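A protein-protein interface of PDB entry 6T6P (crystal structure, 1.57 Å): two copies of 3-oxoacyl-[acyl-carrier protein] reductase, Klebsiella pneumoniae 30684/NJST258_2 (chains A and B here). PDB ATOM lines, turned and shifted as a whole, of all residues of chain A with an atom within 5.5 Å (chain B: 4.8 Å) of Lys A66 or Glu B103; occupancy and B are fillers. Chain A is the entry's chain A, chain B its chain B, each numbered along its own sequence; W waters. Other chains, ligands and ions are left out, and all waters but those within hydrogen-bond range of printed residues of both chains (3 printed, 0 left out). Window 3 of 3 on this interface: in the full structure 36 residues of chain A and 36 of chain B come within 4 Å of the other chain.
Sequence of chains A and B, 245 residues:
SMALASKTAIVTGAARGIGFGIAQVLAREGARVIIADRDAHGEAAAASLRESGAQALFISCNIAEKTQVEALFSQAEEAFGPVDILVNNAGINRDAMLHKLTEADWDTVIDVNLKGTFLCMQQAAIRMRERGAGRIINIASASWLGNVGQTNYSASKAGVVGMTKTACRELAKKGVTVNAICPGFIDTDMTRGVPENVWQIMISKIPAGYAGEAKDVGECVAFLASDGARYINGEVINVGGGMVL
The side-chain carboxylate of Glu B103 lies within salt-bridge range of the side-chain amino group of Lys A115 (2.8 Å). The backbone carbonyl oxygen (O) of Leu B101 lies within hydrogen-bond range of the side-chain amide nitrogen (NE2) of Gln A122. The side-chain carboxylate (OD1) of Asp B107 is in salt-bridge range of the side-chain amino group (NZ) of Lys A115 (2.8 Å).
OE1 of Glu B103 touches CD of Lys A66, 3.8 Å away. Lys A115 touches Trp B106. Phe A118 touches Leu B101. Phe A118 touches Trp B106 (CD2 to CE3, 3.6 Å).
Of chain A, only Lys A66 and Lys A115 come within 4 Å of Glu B103. Printed residues of chain A within 4 Å of Asp B107: Lys A115 (2.8 Å). Printed residues of chain B within 4 Å of Gln A122: Leu B101. Of the printed residues of chain B, Lys A115 touches Glu B103, Trp B106 and Asp B107. The nearest printed residue of chain B that does not touch Lys A66 is Leu B101 (5.0 Å). The nearest residue of chain A that does not touch Glu B103 is Leu A119 (4.9 Å).
Of the 7 printed residues of chain B, 4 touch a printed residue of chain A. Hydrophobic or aromatic side chains of chain B within 4 Å of the printed part of chain A: Leu B101 and Trp B106. Of the 14 printed residues of chain A, 4 touch a printed residue of chain B. Among the printed residues, 7 pairs touch across the chains.
No position is printed for both chains. Of the 7 pairs that touch across the chains among the printed residues, none has its exchanged pair printed and touching as well.
Water W1 lies within hydrogen-bond range of the side-chain carboxylate (OE2) of Glu B103 (2.6 Å), the backbone NH (N) of Lys A66 (2.8 Å) and the backbone carbonyl oxygen (O) of Ala A64 (3.4 Å). Water W2 lies within hydrogen-bond range of the side-chain carboxylate (OD2) of Asp B107 and the side-chain amino group (NZ) of Lys A115. Water W3 lies within hydrogen-bond range of OE1 of Gln A122 (2.8 Å), NZ of Lys A66 (2.8 Å), O of Leu B101 (2.9 Å) and N of Glu B103 (3.3 Å).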
ATOM      1  N   ILE A  63     -19.204  17.434  -8.705  1.00  0.00           N
ATOM      2  CA  ILE A  63     -18.087  17.388  -7.757  1.00  0.00           C
ATOM      3  C   ILE A  63     -16.861  18.228  -8.169  1.00  0.00           C
ATOM      4  O   ILE A  63     -15.974  18.436  -7.355  1.00  0.00           O
ATOM      5  CB  ILE A  63     -17.610  15.940  -7.482  1.00  0.00           C
ATOM      6  CG1 ILE A  63     -17.001  15.262  -8.766  1.00  0.00           C
ATOM      7  CG2 ILE A  63     -18.712  15.189  -6.852  1.00  0.00           C
ATOM      8  CD1 ILE A  63     -16.241  14.008  -8.517  1.00  0.00           C
ATOM      9  N   ALA A  64     -16.841  18.755  -9.388  1.00  0.00           N
ATOM     10  CA  ALA A  64     -15.776  19.659  -9.781  1.00  0.00           C
ATOM     11  C   ALA A  64     -15.841  21.023  -9.116  1.00  0.00           C
ATOM     12  O   ALA A  64     -14.879  21.792  -9.200  1.00  0.00           O
ATOM     13  CB  ALA A  64     -15.721  19.815 -11.297  1.00  0.00           C
ATOM     14  N   GLU A  65     -17.008  21.383  -8.534  1.00  0.00           N
ATOM     15  CA  GLU A  65     -17.153  22.659  -7.858  1.00  0.00           C
ATOM     16  C   GLU A  65     -17.101  22.501  -6.356  1.00  0.00           C
ATOM     17  O   GLU A  65     -18.003  21.851  -5.794  1.00  0.00           O
ATOM     18  CB  GLU A  65     -18.457  23.334  -8.278  1.00  0.00           C
ATOM     19  CG  GLU A  65     -18.443  23.629  -9.748  1.00  0.00           C
ATOM     20  CD  GLU A  65     -19.680  24.358 -10.266  1.00  0.00           C
ATOM     21  OE1 GLU A  65     -20.492  24.892  -9.530  1.00  0.00           O
ATOM     22  OE2 GLU A  65     -19.701  24.467 -11.537  1.00  0.00           O
ATOM     23  N   LYS A  66     -16.118  23.142  -5.721  1.00  0.00           N
ATOM     24  CA  LYS A  66     -15.962  23.006  -4.266  1.00  0.00           C
ATOM     25  C   LYS A  66     -17.232  23.357  -3.475  1.00  0.00           C
ATOM     26  O   LYS A  66     -17.593  22.663  -2.521  1.00  0.00           O
ATOM     27  CB  LYS A  66     -14.788  23.831  -3.753  1.00  0.00           C
ATOM     28  CG  LYS A  66     -14.467  23.646  -2.297  1.00  0.00           C
ATOM     29  CD  LYS A  66     -13.169  24.329  -1.915  1.00  0.00           C
ATOM     30  CE  LYS A  66     -12.894  24.135  -0.441  1.00  0.00           C
ATOM     31  NZ  LYS A  66     -11.696  24.886  -0.036  1.00  0.00           N
ATOM     32  N   THR A  67     -17.919  24.430  -3.871  1.00  0.00           N
ATOM     33  CA  THR A  67     -19.159  24.822  -3.147  1.00  0.00           C
ATOM     34  C   THR A  67     -20.200  23.699  -3.199  1.00  0.00           C
ATOM     35  O   THR A  67     -20.903  23.497  -2.210  1.00  0.00           O
ATOM     36  CB  THR A  67     -19.726  26.088  -3.800  1.00  0.00           C
ATOM     37  OG1 THR A  67     -18.776  27.122  -3.549  1.00  0.00           O
ATOM     38  CG2 THR A  67     -21.053  26.441  -3.139  1.00  0.00           C
ATOM     39  N   GLN A  68     -20.316  23.006  -4.335  1.00  0.00           N
ATOM     40  CA  GLN A  68     -21.281  21.917  -4.460  1.00  0.00           C
ATOM     41  C   GLN A  68     -20.869  20.712  -3.583  1.00  0.00           C
ATOM     42  O   GLN A  68     -21.723  20.072  -2.981  1.00  0.00           O
ATOM     43  CB  GLN A  68     -21.418  21.470  -5.883  1.00  0.00           C
ATOM     44  CG  GLN A  68     -22.052  22.512  -6.747  1.00  0.00           C
ATOM     45  CD  GLN A  68     -22.656  21.962  -8.043  1.00  0.00           C
ATOM     46  OE1 GLN A  68     -22.413  22.561  -9.172  1.00  0.00           O
ATOM     47  NE2 GLN A  68     -23.498  20.974  -7.953  1.00  0.00           N
ATOM     48  N   VAL A  69     -19.567  20.423  -3.533  1.00  0.00           N
ATOM     49  CA  VAL A  69     -19.089  19.354  -2.651  1.00  0.00           C
ATOM     50  C   VAL A  69     -19.318  19.699  -1.186  1.00  0.00           C
ATOM     51  O   VAL A  69     -19.743  18.823  -0.399  1.00  0.00           O
ATOM     52  CB  VAL A  69     -17.558  19.059  -2.910  1.00  0.00           C
ATOM     53  CG1 VAL A  69     -17.023  17.992  -1.984  1.00  0.00           C
ATOM     54  CG2 VAL A  69     -17.369  18.637  -4.338  1.00  0.00           C
ATOM     55  N   GLU A  70     -19.094  20.948  -0.811  1.00  0.00           N
ATOM     56  CA  GLU A  70     -19.382  21.367   0.574  1.00  0.00           C
ATOM     57  C   GLU A  70     -20.866  21.185   0.897  1.00  0.00           C
ATOM     58  O   GLU A  70     -21.226  20.704   1.975  1.00  0.00           O
ATOM     59  CB  GLU A  70     -18.966  22.829   0.786  1.00  0.00           C
ATOM     60  CG  GLU A  70     -17.464  23.017   0.839  1.00  0.00           C
ATOM     61  CD  GLU A  70     -17.014  24.457   0.797  1.00  0.00           C
ATOM     62  OE1 GLU A  70     -15.950  24.767   1.385  1.00  0.00           O
ATOM     63  OE2 GLU A  70     -17.683  25.300   0.138  1.00  0.00           O
ATOM     64  N   ALA A  71     -21.719  21.570  -0.044  1.00  0.00           N
ATOM     65  CA  ALA A  71     -23.154  21.424   0.136  1.00  0.00           C
ATOM     66  C   ALA A  71     -23.591  19.954   0.196  1.00  0.00           C
ATOM     67  O   ALA A  71     -24.471  19.599   0.974  1.00  0.00           O
ATOM     68  CB  ALA A  71     -23.901  22.148  -0.975  1.00  0.00           C
ATOM     69  N   LYS A 115      -9.484  16.630  -9.772  1.00  0.00           N
ATOM     70  CA  LYS A 115      -9.838  17.719  -8.817  1.00  0.00           C
ATOM     71  C   LYS A 115     -11.079  17.369  -8.033  1.00  0.00           C
ATOM     72  O   LYS A 115     -11.131  17.563  -6.812  1.00  0.00           O
ATOM     73  CB  LYS A 115      -9.977  19.072  -9.503  1.00  0.00           C
ATOM     74  CG  LYS A 115     -10.107  20.167  -8.461  1.00  0.00           C
ATOM     75  CD  LYS A 115     -10.134  21.527  -9.138  1.00  0.00           C
ATOM     76  CE  LYS A 115     -10.423  22.645  -8.181  1.00  0.00           C
ATOM     77  NZ  LYS A 115     -10.338  23.971  -8.906  1.00  0.00           N
ATOM     78  N   PHE A 118     -10.269  14.982  -5.353  1.00  0.00           N
ATOM     79  CA  PHE A 118      -9.579  15.708  -4.270  1.00  0.00           C
ATOM     80  C   PHE A 118     -10.571  16.462  -3.394  1.00  0.00           C
ATOM     81  O   PHE A 118     -10.504  16.415  -2.175  1.00  0.00           O
ATOM     82  CB  PHE A 118      -8.548  16.688  -4.879  1.00  0.00           C
ATOM     83  CG  PHE A 118      -8.244  17.881  -4.007  1.00  0.00           C
ATOM     84  CD1 PHE A 118      -7.683  17.755  -2.737  1.00  0.00           C
ATOM     85  CD2 PHE A 118      -8.551  19.164  -4.459  1.00  0.00           C
ATOM     86  CE1 PHE A 118      -7.433  18.859  -1.958  1.00  0.00           C
ATOM     87  CE2 PHE A 118      -8.297  20.263  -3.702  1.00  0.00           C
ATOM     88  CZ  PHE A 118      -7.735  20.137  -2.421  1.00  0.00           C
ATOM     89  N   LEU A 119     -11.476  17.231  -3.998  1.00  0.00           N
ATOM     90  CA  LEU A 119     -12.378  18.057  -3.212  1.00  0.00           C
ATOM     91  C   LEU A 119     -13.247  17.227  -2.267  1.00  0.00           C
ATOM     92  O   LEU A 119     -13.480  17.593  -1.131  1.00  0.00           O
ATOM     93  CB  LEU A 119     -13.240  18.933  -4.131  1.00  0.00           C
ATOM     94  CG  LEU A 119     -12.512  19.997  -4.919  1.00  0.00           C
ATOM     95  CD1 LEU A 119     -13.516  20.560  -5.953  1.00  0.00           C
ATOM     96  CD2 LEU A 119     -11.928  21.078  -4.020  1.00  0.00           C
ATOM     97  N   GLN A 122     -11.130  15.838   0.522  1.00  0.00           N
ATOM     98  CA  GLN A 122     -10.817  16.891   1.476  1.00  0.00           C
ATOM     99  C   GLN A 122     -11.978  17.104   2.444  1.00  0.00           C
ATOM    100  O   GLN A 122     -11.766  17.246   3.671  1.00  0.00           O
ATOM    101  CB  GLN A 122     -10.477  18.192   0.763  1.00  0.00           C
ATOM    102  CG  GLN A 122     -10.270  19.377   1.653  1.00  0.00           C
ATOM    103  CD  GLN A 122      -9.727  20.568   0.877  1.00  0.00           C
ATOM    104  OE1 GLN A 122     -10.448  21.167   0.045  1.00  0.00           O
ATOM    105  NE2 GLN A 122      -8.475  20.927   1.149  1.00  0.00           N
ATOM    106  N   GLN A 123     -13.203  17.161   1.929  1.00  0.00           N
ATOM    107  CA  GLN A 123     -14.354  17.317   2.827  1.00  0.00           C
ATOM    108  C   GLN A 123     -14.491  16.135   3.802  1.00  0.00           C
ATOM    109  O   GLN A 123     -14.897  16.310   4.954  1.00  0.00           O
ATOM    110  CB  GLN A 123     -15.639  17.509   2.049  1.00  0.00           C
ATOM    111  CG  GLN A 123     -15.740  18.875   1.371  1.00  0.00           C
ATOM    112  CD  GLN A 123     -15.566  20.016   2.303  1.00  0.00           C
ATOM    113  OE1 GLN A 123     -16.305  20.160   3.303  1.00  0.00           O
ATOM    114  NE2 GLN A 123     -14.644  20.905   1.977  1.00  0.00           N
ATOM    115  N   LEU B 101      -5.326  22.097   2.151  1.00  0.00           N
ATOM    116  CA  LEU B 101      -4.837  22.492   0.828  1.00  0.00           C
ATOM    117  C   LEU B 101      -5.826  23.433   0.147  1.00  0.00           C
ATOM    118  O   LEU B 101      -7.017  23.093  -0.028  1.00  0.00           O
ATOM    119  CB  LEU B 101      -4.601  21.293  -0.039  1.00  0.00           C
ATOM    120  CG  LEU B 101      -4.160  21.565  -1.475  1.00  0.00           C
ATOM    121  CD1 LEU B 101      -2.833  22.284  -1.507  1.00  0.00           C
ATOM    122  CD2 LEU B 101      -4.073  20.289  -2.301  1.00  0.00           C
ATOM    123  N   THR B 102      -5.402  24.638  -0.193  1.00  0.00           N
ATOM    124  CA  THR B 102      -6.271  25.561  -0.839  1.00  0.00           C
ATOM    125  C   THR B 102      -6.488  25.158  -2.290  1.00  0.00           C
ATOM    126  O   THR B 102      -5.676  24.514  -2.943  1.00  0.00           O
ATOM    127  CB  THR B 102      -5.740  27.026  -0.795  1.00  0.00           C
ATOM    128  OG1 THR B 102      -4.545  27.118  -1.613  1.00  0.00           O
ATOM    129  CG2 THR B 102      -5.507  27.496   0.590  1.00  0.00           C
ATOM    130  N   GLU B 103      -7.612  25.622  -2.806  1.00  0.00           N
ATOM    131  CA  GLU B 103      -7.882  25.383  -4.208  1.00  0.00           C
ATOM    132  C   GLU B 103      -6.804  26.012  -5.122  1.00  0.00           C
ATOM    133  O   GLU B 103      -6.408  25.428  -6.139  1.00  0.00           O
ATOM    134  CB  GLU B 103      -9.293  25.893  -4.487  1.00  0.00           C
ATOM    135  CG  GLU B 103      -9.848  25.455  -5.762  1.00  0.00           C
ATOM    136  CD  GLU B 103     -11.397  25.636  -5.825  1.00  0.00           C
ATOM    137  OE1 GLU B 103     -12.054  26.329  -4.970  1.00  0.00           O
ATOM    138  OE2 GLU B 103     -11.832  25.284  -6.939  1.00  0.00           O
ATOM    139  N   ALA B 104      -6.340  27.201  -4.761  1.00  0.00           N
ATOM    140  CA  ALA B 104      -5.306  27.853  -5.580  1.00  0.00           C
ATOM    141  C   ALA B 104      -4.027  27.011  -5.614  1.00  0.00           C
ATOM    142  O   ALA B 104      -3.379  26.878  -6.664  1.00  0.00           O
ATOM    143  CB  ALA B 104      -5.002  29.251  -5.086  1.00  0.00           C
ATOM    144  N   ASP B 105      -3.630  26.470  -4.460  1.00  0.00           N
ATOM    145  CA  ASP B 105      -2.414  25.677  -4.391  1.00  0.00           C
ATOM    146  C   ASP B 105      -2.541  24.334  -5.141  1.00  0.00           C
ATOM    147  O   ASP B 105      -1.597  23.817  -5.738  1.00  0.00           O
ATOM    148  CB  ASP B 105      -1.958  25.500  -2.946  1.00  0.00           C
ATOM    149  CG  ASP B 105      -1.246  26.731  -2.375  1.00  0.00           C
ATOM    150  OD1 ASP B 105      -0.967  27.719  -3.090  1.00  0.00           O
ATOM    151  OD2 ASP B 105      -0.987  26.704  -1.147  1.00  0.00           O
ATOM    152  N   TRP B 106      -3.744  23.741  -5.096  1.00  0.00           N
ATOM    153  CA  TRP B 106      -4.078  22.593  -5.922  1.00  0.00           C
ATOM    154  C   TRP B 106      -3.906  22.963  -7.393  1.00  0.00           C
ATOM    155  O   TRP B 106      -3.173  22.286  -8.152  1.00  0.00           O
ATOM    156  CB  TRP B 106      -5.526  22.098  -5.623  1.00  0.00           C
ATOM    157  CG  TRP B 106      -5.936  21.114  -6.673  1.00  0.00           C
ATOM    158  CD1 TRP B 106      -6.559  21.422  -7.851  1.00  0.00           C
ATOM    159  CD2 TRP B 106      -5.698  19.700  -6.709  1.00  0.00           C
ATOM    160  NE1 TRP B 106      -6.691  20.316  -8.623  1.00  0.00           N
ATOM    161  CE2 TRP B 106      -6.240  19.225  -7.927  1.00  0.00           C
ATOM    162  CE3 TRP B 106      -5.183  18.761  -5.789  1.00  0.00           C
ATOM    163  CZ2 TRP B 106      -6.170  17.911  -8.300  1.00  0.00           C
ATOM    164  CZ3 TRP B 106      -5.123  17.445  -6.151  1.00  0.00           C
ATOM    165  CH2 TRP B 106      -5.593  17.028  -7.418  1.00  0.00           C
ATOM    166  N   ASP B 107      -4.602  24.011  -7.798  1.00  0.00           N
ATOM    167  CA  ASP B 107      -4.676  24.359  -9.199  1.00  0.00           C
ATOM    168  C   ASP B 107      -3.300  24.641  -9.779  1.00  0.00           C
ATOM    169  O   ASP B 107      -2.981  24.179 -10.898  1.00  0.00           O
ATOM    170  CB  ASP B 107      -5.545  25.593  -9.447  1.00  0.00           C
ATOM    171  CG  ASP B 107      -7.038  25.358  -9.276  1.00  0.00           C
ATOM    172  OD1 ASP B 107      -7.554  24.199  -9.331  1.00  0.00           O
ATOM    173  OD2 ASP B 107      -7.752  26.420  -9.094  1.00  0.00           O
HETATM  174  O   HOH W   1     -14.280  24.553  -7.260  1.00  0.00           O
HETATM  175  O   HOH W   2     -10.060  26.568 -10.413  1.00  0.00           O
HETATM  176  O   HOH W   3      -9.637  23.433  -1.299  1.00  0.00           O
